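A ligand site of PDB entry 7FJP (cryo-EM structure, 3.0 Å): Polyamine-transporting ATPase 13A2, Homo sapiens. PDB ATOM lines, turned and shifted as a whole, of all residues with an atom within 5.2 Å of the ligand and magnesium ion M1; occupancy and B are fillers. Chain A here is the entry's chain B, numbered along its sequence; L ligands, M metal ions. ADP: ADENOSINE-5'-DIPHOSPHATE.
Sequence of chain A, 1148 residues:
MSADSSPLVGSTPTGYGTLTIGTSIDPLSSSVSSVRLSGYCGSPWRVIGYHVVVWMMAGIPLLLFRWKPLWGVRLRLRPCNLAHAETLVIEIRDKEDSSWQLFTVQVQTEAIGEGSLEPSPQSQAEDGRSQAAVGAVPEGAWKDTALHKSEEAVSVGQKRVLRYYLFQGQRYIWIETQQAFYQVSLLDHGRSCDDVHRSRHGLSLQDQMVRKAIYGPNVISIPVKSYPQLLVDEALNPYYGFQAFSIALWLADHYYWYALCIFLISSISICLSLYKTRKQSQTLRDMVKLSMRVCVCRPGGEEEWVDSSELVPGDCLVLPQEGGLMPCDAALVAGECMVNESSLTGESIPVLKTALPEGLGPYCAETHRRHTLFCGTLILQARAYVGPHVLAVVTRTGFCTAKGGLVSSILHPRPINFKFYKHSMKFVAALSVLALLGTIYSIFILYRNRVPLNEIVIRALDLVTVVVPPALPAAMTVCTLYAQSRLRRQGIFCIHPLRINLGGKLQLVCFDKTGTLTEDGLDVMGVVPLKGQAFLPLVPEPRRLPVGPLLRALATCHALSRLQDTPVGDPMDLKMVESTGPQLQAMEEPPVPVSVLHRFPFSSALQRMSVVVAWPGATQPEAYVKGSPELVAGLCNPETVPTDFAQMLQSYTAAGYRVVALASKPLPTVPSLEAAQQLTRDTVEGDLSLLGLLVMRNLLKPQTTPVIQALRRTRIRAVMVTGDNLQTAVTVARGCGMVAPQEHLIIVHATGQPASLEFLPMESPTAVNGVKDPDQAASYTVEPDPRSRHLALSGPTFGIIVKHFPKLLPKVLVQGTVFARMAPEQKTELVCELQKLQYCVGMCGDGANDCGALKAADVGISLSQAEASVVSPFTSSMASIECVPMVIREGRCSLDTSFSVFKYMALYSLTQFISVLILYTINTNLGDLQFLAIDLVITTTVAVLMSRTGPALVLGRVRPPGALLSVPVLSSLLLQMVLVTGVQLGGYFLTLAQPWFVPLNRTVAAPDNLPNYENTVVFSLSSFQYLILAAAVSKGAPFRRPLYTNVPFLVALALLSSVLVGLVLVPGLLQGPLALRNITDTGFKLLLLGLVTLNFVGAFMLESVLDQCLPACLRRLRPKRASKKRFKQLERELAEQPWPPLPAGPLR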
ATOM      1  N   LYS A 513      19.822 -15.142  30.965  1.00  0.00           N
ATOM      2  CA  LYS A 513      20.484 -14.881  32.242  1.00  0.00           C
ATOM      3  C   LYS A 513      20.018 -13.818  33.246  1.00  0.00           C
ATOM      4  O   LYS A 513      19.998 -14.102  34.437  1.00  0.00           O
ATOM      5  CB  LYS A 513      21.980 -14.679  31.993  1.00  0.00           C
ATOM      6  CG  LYS A 513      22.762 -14.325  33.245  1.00  0.00           C
ATOM      7  CD  LYS A 513      24.194 -13.978  32.918  1.00  0.00           C
ATOM      8  CE  LYS A 513      24.298 -12.624  32.234  1.00  0.00           C
ATOM      9  NZ  LYS A 513      23.733 -11.554  33.096  1.00  0.00           N
ATOM     10  N   THR A 514      19.636 -12.628  32.811  1.00  0.00           N
ATOM     11  CA  THR A 514      19.322 -11.584  33.770  1.00  0.00           C
ATOM     12  C   THR A 514      17.832 -11.570  34.065  1.00  0.00           C
ATOM     13  O   THR A 514      17.016 -11.486  33.150  1.00  0.00           O
ATOM     14  CB  THR A 514      19.772 -10.222  33.249  1.00  0.00           C
ATOM     15  OG1 THR A 514      21.182 -10.249  33.004  1.00  0.00           O
ATOM     16  CG2 THR A 514      19.466  -9.139  34.253  1.00  0.00           C
ATOM     17  N   ASP A 570      13.531   1.617  35.094  1.00  0.00           N
ATOM     18  CA  ASP A 570      14.424   0.487  34.865  1.00  0.00           C
ATOM     19  C   ASP A 570      15.139   0.133  36.165  1.00  0.00           C
ATOM     20  O   ASP A 570      15.602   1.027  36.875  1.00  0.00           O
ATOM     21  CB  ASP A 570      15.438   0.872  33.783  1.00  0.00           C
ATOM     22  CG  ASP A 570      16.139  -0.311  33.142  1.00  0.00           C
ATOM     23  OD1 ASP A 570      15.835  -1.472  33.459  1.00  0.00           O
ATOM     24  OD2 ASP A 570      17.025  -0.081  32.286  1.00  0.00           O
ATOM     25  N   MET A 572      18.069  -0.980  36.569  1.00  0.00           N
ATOM     26  CA  MET A 572      19.407  -0.392  36.564  1.00  0.00           C
ATOM     27  C   MET A 572      19.344   1.089  36.884  1.00  0.00           C
ATOM     28  O   MET A 572      20.172   1.599  37.662  1.00  0.00           O
ATOM     29  CB  MET A 572      20.075  -0.616  35.207  1.00  0.00           C
ATOM     30  CG  MET A 572      21.495  -0.109  35.142  1.00  0.00           C
ATOM     31  SD  MET A 572      22.226  -0.324  33.517  1.00  0.00           S
ATOM     32  CE  MET A 572      22.411  -2.099  33.459  1.00  0.00           C
ATOM     33  N   ASP A 573      18.368   1.800  36.323  1.00  0.00           N
ATOM     34  CA  ASP A 573      18.302   3.243  36.493  1.00  0.00           C
ATOM     35  C   ASP A 573      17.807   3.631  37.877  1.00  0.00           C
ATOM     36  O   ASP A 573      18.097   4.731  38.349  1.00  0.00           O
ATOM     37  CB  ASP A 573      17.398   3.863  35.425  1.00  0.00           C
ATOM     38  CG  ASP A 573      17.915   3.637  34.027  1.00  0.00           C
ATOM     39  OD1 ASP A 573      19.140   3.448  33.881  1.00  0.00           O
ATOM     40  OD2 ASP A 573      17.115   3.666  33.081  1.00  0.00           O
ATOM     41  N   PHE A 602      16.539   3.511  25.651  1.00  0.00           N
ATOM     42  CA  PHE A 602      17.263   2.244  25.551  1.00  0.00           C
ATOM     43  C   PHE A 602      16.485   1.253  24.702  1.00  0.00           C
ATOM     44  O   PHE A 602      15.334   0.925  25.009  1.00  0.00           O
ATOM     45  CB  PHE A 602      17.539   1.659  26.933  1.00  0.00           C
ATOM     46  CG  PHE A 602      18.160   0.300  26.886  1.00  0.00           C
ATOM     47  CD1 PHE A 602      19.459   0.138  26.444  1.00  0.00           C
ATOM     48  CD2 PHE A 602      17.437  -0.823  27.263  1.00  0.00           C
ATOM     49  CE1 PHE A 602      20.037  -1.114  26.381  1.00  0.00           C
ATOM     50  CE2 PHE A 602      18.015  -2.074  27.199  1.00  0.00           C
ATOM     51  CZ  PHE A 602      19.312  -2.212  26.759  1.00  0.00           C
ATOM     52  N   SER A 604      17.156  -2.730  23.187  1.00  0.00           N
ATOM     53  CA  SER A 604      18.010  -3.882  23.475  1.00  0.00           C
ATOM     54  C   SER A 604      18.920  -4.247  22.317  1.00  0.00           C
ATOM     55  O   SER A 604      19.964  -4.868  22.535  1.00  0.00           O
ATOM     56  CB  SER A 604      17.141  -5.081  23.848  1.00  0.00           C
ATOM     57  OG  SER A 604      17.942  -6.221  24.086  1.00  0.00           O
ATOM     58  N   GLN A 607      21.918  -1.339  22.544  1.00  0.00           N
ATOM     59  CA  GLN A 607      22.733  -1.549  23.737  1.00  0.00           C
ATOM     60  C   GLN A 607      23.281  -0.271  24.344  1.00  0.00           C
ATOM     61  O   GLN A 607      24.364  -0.278  24.935  1.00  0.00           O
ATOM     62  CB  GLN A 607      23.880  -2.525  23.443  1.00  0.00           C
ATOM     63  CG  GLN A 607      23.423  -3.940  23.141  1.00  0.00           C
ATOM     64  CD  GLN A 607      24.566  -4.850  22.745  1.00  0.00           C
ATOM     65  OE1 GLN A 607      25.701  -4.403  22.592  1.00  0.00           O
ATOM     66  NE2 GLN A 607      24.272  -6.125  22.583  1.00  0.00           N
ATOM     67  N   ARG A 608      22.563   0.839  24.217  1.00  0.00           N
ATOM     68  CA  ARG A 608      23.059   2.118  24.725  1.00  0.00           C
ATOM     69  C   ARG A 608      21.887   3.039  24.981  1.00  0.00           C
ATOM     70  O   ARG A 608      20.741   2.735  24.645  1.00  0.00           O
ATOM     71  CB  ARG A 608      24.072   2.744  23.753  1.00  0.00           C
ATOM     72  CG  ARG A 608      23.526   3.000  22.378  1.00  0.00           C
ATOM     73  CD  ARG A 608      24.643   3.399  21.445  1.00  0.00           C
ATOM     74  NE  ARG A 608      24.148   3.682  20.099  1.00  0.00           N
ATOM     75  CZ  ARG A 608      24.000   2.761  19.153  1.00  0.00           C
ATOM     76  NH1 ARG A 608      24.318   1.500  19.401  1.00  0.00           N
ATOM     77  NH2 ARG A 608      23.552   3.103  17.959  1.00  0.00           N
ATOM     78  N   MET A 609      22.191   4.184  25.597  1.00  0.00           N
ATOM     79  CA  MET A 609      21.165   5.153  25.968  1.00  0.00           C
ATOM     80  C   MET A 609      21.811   6.520  26.133  1.00  0.00           C
ATOM     81  O   MET A 609      22.790   6.651  26.851  1.00  0.00           O
ATOM     82  CB  MET A 609      20.482   4.759  27.275  1.00  0.00           C
ATOM     83  CG  MET A 609      19.411   5.721  27.639  1.00  0.00           C
ATOM     84  SD  MET A 609      18.508   5.392  29.134  1.00  0.00           S
ATOM     85  CE  MET A 609      17.468   6.842  29.080  1.00  0.00           C
ATOM     86  N   LYS A 626      25.258   5.955  28.032  1.00  0.00           N
ATOM     87  CA  LYS A 626      25.391   4.834  28.945  1.00  0.00           C
ATOM     88  C   LYS A 626      25.081   3.548  28.195  1.00  0.00           C
ATOM     89  O   LYS A 626      23.943   3.372  27.751  1.00  0.00           O
ATOM     90  CB  LYS A 626      24.451   4.983  30.136  1.00  0.00           C
ATOM     91  CG  LYS A 626      24.523   3.827  31.111  1.00  0.00           C
ATOM     92  CD  LYS A 626      23.627   4.077  32.292  1.00  0.00           C
ATOM     93  CE  LYS A 626      22.186   3.930  31.885  1.00  0.00           C
ATOM     94  NZ  LYS A 626      21.265   3.987  33.036  1.00  0.00           N
ATOM     95  N   GLY A 627      26.064   2.676  28.063  1.00  0.00           N
ATOM     96  CA  GLY A 627      25.835   1.457  27.323  1.00  0.00           C
ATOM     97  C   GLY A 627      26.767   0.347  27.739  1.00  0.00           C
ATOM     98  O   GLY A 627      27.420   0.425  28.789  1.00  0.00           O
ATOM     99  N   SER A 628      26.826  -0.690  26.908  1.00  0.00           N
ATOM    100  CA  SER A 628      27.706  -1.809  27.175  1.00  0.00           C
ATOM    101  C   SER A 628      29.155  -1.383  26.950  1.00  0.00           C
ATOM    102  O   SER A 628      29.428  -0.553  26.080  1.00  0.00           O
ATOM    103  CB  SER A 628      27.347  -2.990  26.281  1.00  0.00           C
ATOM    104  OG  SER A 628      27.604  -2.702  24.928  1.00  0.00           O
ATOM    105  N   PRO A 629      30.111  -1.917  27.731  1.00  0.00           N
ATOM    106  CA  PRO A 629      31.468  -1.340  27.732  1.00  0.00           C
ATOM    107  C   PRO A 629      32.257  -1.570  26.453  1.00  0.00           C
ATOM    108  O   PRO A 629      33.023  -0.694  26.073  1.00  0.00           O
ATOM    109  CB  PRO A 629      32.133  -2.021  28.932  1.00  0.00           C
ATOM    110  CG  PRO A 629      31.010  -2.482  29.778  1.00  0.00           C
ATOM    111  CD  PRO A 629      29.935  -2.873  28.836  1.00  0.00           C
ATOM    112  N   ARG A 658      28.186  -7.005  36.790  1.00  0.00           N
ATOM    113  CA  ARG A 658      27.416  -6.395  35.715  1.00  0.00           C
ATOM    114  C   ARG A 658      27.991  -5.003  35.478  1.00  0.00           C
ATOM    115  O   ARG A 658      27.816  -4.107  36.317  1.00  0.00           O
ATOM    116  CB  ARG A 658      25.944  -6.313  36.104  1.00  0.00           C
ATOM    117  CG  ARG A 658      25.021  -5.741  35.055  1.00  0.00           C
ATOM    118  CD  ARG A 658      24.748  -6.755  33.978  1.00  0.00           C
ATOM    119  NE  ARG A 658      23.824  -6.254  32.962  1.00  0.00           N
ATOM    120  CZ  ARG A 658      22.507  -6.300  33.069  1.00  0.00           C
ATOM    121  NH1 ARG A 658      21.948  -6.805  34.145  1.00  0.00           N
ATOM    122  NH2 ARG A 658      21.747  -5.828  32.093  1.00  0.00           N
ATOM    123  N   VAL A 659      28.673  -4.814  34.359  1.00  0.00           N
ATOM    124  CA  VAL A 659      29.441  -3.595  34.100  1.00  0.00           C
ATOM    125  C   VAL A 659      28.849  -2.887  32.893  1.00  0.00           C
ATOM    126  O   VAL A 659      28.621  -3.511  31.854  1.00  0.00           O
ATOM    127  CB  VAL A 659      30.936  -3.907  33.877  1.00  0.00           C
ATOM    128  CG1 VAL A 659      31.712  -2.635  33.627  1.00  0.00           C
ATOM    129  CG2 VAL A 659      31.509  -4.661  35.060  1.00  0.00           C
ATOM    130  N   VAL A 660      28.579  -1.591  33.043  1.00  0.00           N
ATOM    131  CA  VAL A 660      28.234  -0.708  31.936  1.00  0.00           C
ATOM    132  C   VAL A 660      29.215   0.455  31.936  1.00  0.00           C
ATOM    133  O   VAL A 660      29.912   0.707  32.929  1.00  0.00           O
ATOM    134  CB  VAL A 660      26.787  -0.197  32.012  1.00  0.00           C
ATOM    135  CG1 VAL A 660      25.799  -1.340  31.928  1.00  0.00           C
ATOM    136  CG2 VAL A 660      26.572   0.612  33.272  1.00  0.00           C
ATOM    137  N   THR A 722      21.849 -15.068  26.271  1.00  0.00           N
ATOM    138  CA  THR A 722      21.712 -13.766  26.902  1.00  0.00           C
ATOM    139  C   THR A 722      22.284 -12.693  25.993  1.00  0.00           C
ATOM    140  O   THR A 722      22.967 -12.978  25.009  1.00  0.00           O
ATOM    141  CB  THR A 722      22.414 -13.730  28.261  1.00  0.00           C
ATOM    142  OG1 THR A 722      22.109 -12.505  28.925  1.00  0.00           O
ATOM    143  CG2 THR A 722      23.918 -13.852  28.097  1.00  0.00           C
ATOM    144  N   GLY A 723      21.977 -11.440  26.311  1.00  0.00           N
ATOM    145  CA  GLY A 723      22.560 -10.292  25.652  1.00  0.00           C
ATOM    146  C   GLY A 723      23.635  -9.604  26.444  1.00  0.00           C
ATOM    147  O   GLY A 723      24.176  -8.590  25.992  1.00  0.00           O
ATOM    148  N   ASP A 724      23.970 -10.133  27.616  1.00  0.00           N
ATOM    149  CA  ASP A 724      24.962  -9.576  28.524  1.00  0.00           C
ATOM    150  C   ASP A 724      26.360  -9.970  28.050  1.00  0.00           C
ATOM    151  O   ASP A 724      26.528 -10.621  27.023  1.00  0.00           O
ATOM    152  CB  ASP A 724      24.645 -10.052  29.940  1.00  0.00           C
ATOM    153  CG  ASP A 724      25.254  -9.191  31.010  1.00  0.00           C
ATOM    154  OD1 ASP A 724      25.967  -8.228  30.683  1.00  0.00           O
ATOM    155  OD2 ASP A 724      25.009  -9.493  32.201  1.00  0.00           O
ATOM    156  N   ASN A 725      27.376  -9.560  28.809  1.00  0.00           N
ATOM    157  CA  ASN A 725      28.779  -9.729  28.430  1.00  0.00           C
ATOM    158  C   ASN A 725      29.149 -11.208  28.435  1.00  0.00           C
ATOM    159  O   ASN A 725      28.518 -12.037  29.087  1.00  0.00           O
ATOM    160  CB  ASN A 725      29.666  -8.936  29.391  1.00  0.00           C
ATOM    161  CG  ASN A 725      31.077  -8.753  28.872  1.00  0.00           C
ATOM    162  OD1 ASN A 725      31.421  -9.215  27.782  1.00  0.00           O
ATOM    163  ND2 ASN A 725      31.904  -8.080  29.657  1.00  0.00           N
ATOM    164  N   ARG A 821      25.901 -11.676  24.203  1.00  0.00           N
ATOM    165  CA  ARG A 821      25.745 -10.475  23.372  1.00  0.00           C
ATOM    166  C   ARG A 821      24.804 -10.714  22.196  1.00  0.00           C
ATOM    167  O   ARG A 821      25.007 -10.182  21.100  1.00  0.00           O
ATOM    168  CB  ARG A 821      27.093  -9.931  22.897  1.00  0.00           C
ATOM    169  CG  ARG A 821      27.953  -9.384  24.002  1.00  0.00           C
ATOM    170  CD  ARG A 821      27.256  -8.189  24.573  1.00  0.00           C
ATOM    171  NE  ARG A 821      28.000  -7.572  25.661  1.00  0.00           N
ATOM    172  CZ  ARG A 821      27.503  -6.621  26.440  1.00  0.00           C
ATOM    173  NH1 ARG A 821      26.272  -6.204  26.227  1.00  0.00           N
ATOM    174  NH2 ARG A 821      28.226  -6.104  27.416  1.00  0.00           N
ATOM    175  N   MET A 822      23.759 -11.498  22.425  1.00  0.00           N
ATOM    176  CA  MET A 822      22.846 -11.888  21.370  1.00  0.00           C
ATOM    177  C   MET A 822      21.795 -10.809  21.172  1.00  0.00           C
ATOM    178  O   MET A 822      21.157 -10.364  22.134  1.00  0.00           O
ATOM    179  CB  MET A 822      22.174 -13.225  21.695  1.00  0.00           C
ATOM    180  CG  MET A 822      23.150 -14.381  21.755  1.00  0.00           C
ATOM    181  SD  MET A 822      23.980 -14.752  20.201  1.00  0.00           S
ATOM    182  CE  MET A 822      22.666 -15.561  19.318  1.00  0.00           C
ATOM    183  N   ASN A 849      13.107  -8.766  24.891  1.00  0.00           N
ATOM    184  CA  ASN A 849      14.091  -9.266  23.954  1.00  0.00           C
ATOM    185  C   ASN A 849      13.930 -10.754  23.669  1.00  0.00           C
ATOM    186  O   ASN A 849      14.531 -11.247  22.712  1.00  0.00           O
ATOM    187  CB  ASN A 849      15.504  -8.978  24.466  1.00  0.00           C
ATOM    188  CG  ASN A 849      15.750  -9.476  25.866  1.00  0.00           C
ATOM    189  OD1 ASN A 849      14.879 -10.056  26.508  1.00  0.00           O
ATOM    190  ND2 ASN A 849      16.960  -9.252  26.362  1.00  0.00           N
HETATM  191  PB  ADP L   1      20.268  -8.207  29.621  1.00  0.00           P
HETATM  192  O1B ADP L   1      21.156  -8.031  30.823  1.00  0.00           O
HETATM  193  O2B ADP L   1      18.831  -7.826  29.860  1.00  0.00           O
HETATM  194  O3B ADP L   1      20.464  -9.517  28.904  1.00  0.00           O
HETATM  195  PA  ADP L   1      20.035  -6.445  27.363  1.00  0.00           P
HETATM  196  O1A ADP L   1      18.740  -5.820  27.818  1.00  0.00           O
HETATM  197  O2A ADP L   1      20.042  -7.414  26.209  1.00  0.00           O
HETATM  198  O3A ADP L   1      20.836  -7.081  28.614  1.00  0.00           O
HETATM  199  O5' ADP L   1      21.048  -5.252  27.003  1.00  0.00           O
HETATM  200  C5' ADP L   1      22.274  -5.512  26.338  1.00  0.00           C
HETATM  201  C4' ADP L   1      23.348  -4.666  27.002  1.00  0.00           C
HETATM  202  O4' ADP L   1      22.829  -3.366  27.259  1.00  0.00           O
HETATM  203  C3' ADP L   1      23.762  -5.239  28.342  1.00  0.00           C
HETATM  204  O3' ADP L   1      25.116  -5.671  28.278  1.00  0.00           O
HETATM  205  C2' ADP L   1      23.679  -4.113  29.333  1.00  0.00           C
HETATM  206  O2' ADP L   1      24.986  -3.879  29.879  1.00  0.00           O
HETATM  207  C1' ADP L   1      23.227  -2.912  28.545  1.00  0.00           C
HETATM  208  N9  ADP L   1      22.061  -2.303  29.211  1.00  0.00           N
HETATM  209  C8  ADP L   1      21.060  -2.989  29.792  1.00  0.00           C
HETATM  210  N7  ADP L   1      20.148  -2.141  30.327  1.00  0.00           N
HETATM  211  C5  ADP L   1      20.583  -0.887  30.091  1.00  0.00           C
HETATM  212  C6  ADP L   1      20.094   0.476  30.386  1.00  0.00           C
HETATM  213  N6  ADP L   1      18.942   0.680  31.056  1.00  0.00           N
HETATM  214  N1  ADP L   1      20.843   1.504  29.962  1.00  0.00           N
HETATM  215  C2  ADP L   1      21.992   1.324  29.294  1.00  0.00           C
HETATM  216  N3  ADP L   1      22.492   0.118  28.992  1.00  0.00           N
HETATM  217  C4  ADP L   1      21.844  -1.002  29.361  1.00  0.00           C
HETATM  218 MG    MG M   1      17.921  -6.266  30.610  1.00  0.00          MG
HETATM  219 MG    MG M   2      15.194 -10.296  31.288  1.00  0.00          MG
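N6 of the ligand lies within hydrogen-bond range of OD2 of Asp 570, at 2.4 Å. The side-chain hydroxyl (OG1) of Thr 514 is in hydrogen-bond range of an oxygen (O1B) of the ligand. The guanidinium group (NH2) of Arg 658 is in salt-bridge range of an oxygen (O1B) of the ligand (2.6 Å). NH1 of Arg 821 is in hydrogen-bond range of O3' of the ligand, 2.4 Å away. O3B of the ligand lies within hydrogen-bond range of OG1 of Thr 722, 3.4 Å away. O2A of the ligand lies within hydrogen-bond range of OG of Ser 604, at 3.2 Å.
Met 572 touches the ligand (SD to C5, 3.8 Å). Asp 573 touches the ligand (OD1 to N6, 3.96 Å). CE1 of Phe 602 touches C4 of the ligand, at 3.5 Å. Gln 607 touches the ligand (CG to C5', 3.7 Å). O of Lys 626 touches C2 of the ligand (3.2 Å). CA of Gly 627 touches N3 of the ligand, 3.97 Å away. CG1 of Val 660 touches O2' of the ligand, 3.4 Å away. Gly 723 touches the ligand (N to O3B, 3.6 Å). Asp 724 touches the ligand (OD1 to O3', 3.6 Å). ND2 of Asn 849 touches O2A of the ligand, 3.6 Å away. Of the 24 residues printed, 16 come within 4 Å of the ligand.
No residue comes within 4 Å of magnesium ion M1. The nearest printed residue that does not touch magnesium ion M1 is Arg 658 (4.1 Å).
N of Arg 821 lies within hydrogen-bond range of O of Asp 724 (3.1 Å). The side-chain hydroxyl (OG1) of Thr 722 sits at hydrogen-bond distance from the backbone NH (N) of Asp 724. The guanidinium group of Arg 821 is in hydrogen-bond range of the backbone carbonyl oxygen of Gly 723 (3.2 Å). N of Arg 821 is in hydrogen-bond range of O of Thr 722 (3.3 Å). The backbone NH (N) of Ser 628 is in hydrogen-bond range of the backbone carbonyl oxygen (O) of Gln 607. The side-chain amino group (NZ) of Lys 513 is in salt-bridge range of the side-chain carboxylate (OD2) of Asp 724, at 2.6 Å. The backbone carbonyl oxygen (O) of Met 609 sits at hydrogen-bond distance from the backbone NH (N) of Lys 626 (2.8 Å). The guanidinium group (NE) of Arg 658 is in salt-bridge range of the side-chain carboxylate (OD2) of Asp 724, at 3.5 Å.
O2B of the ligand binds magnesium ion M1.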
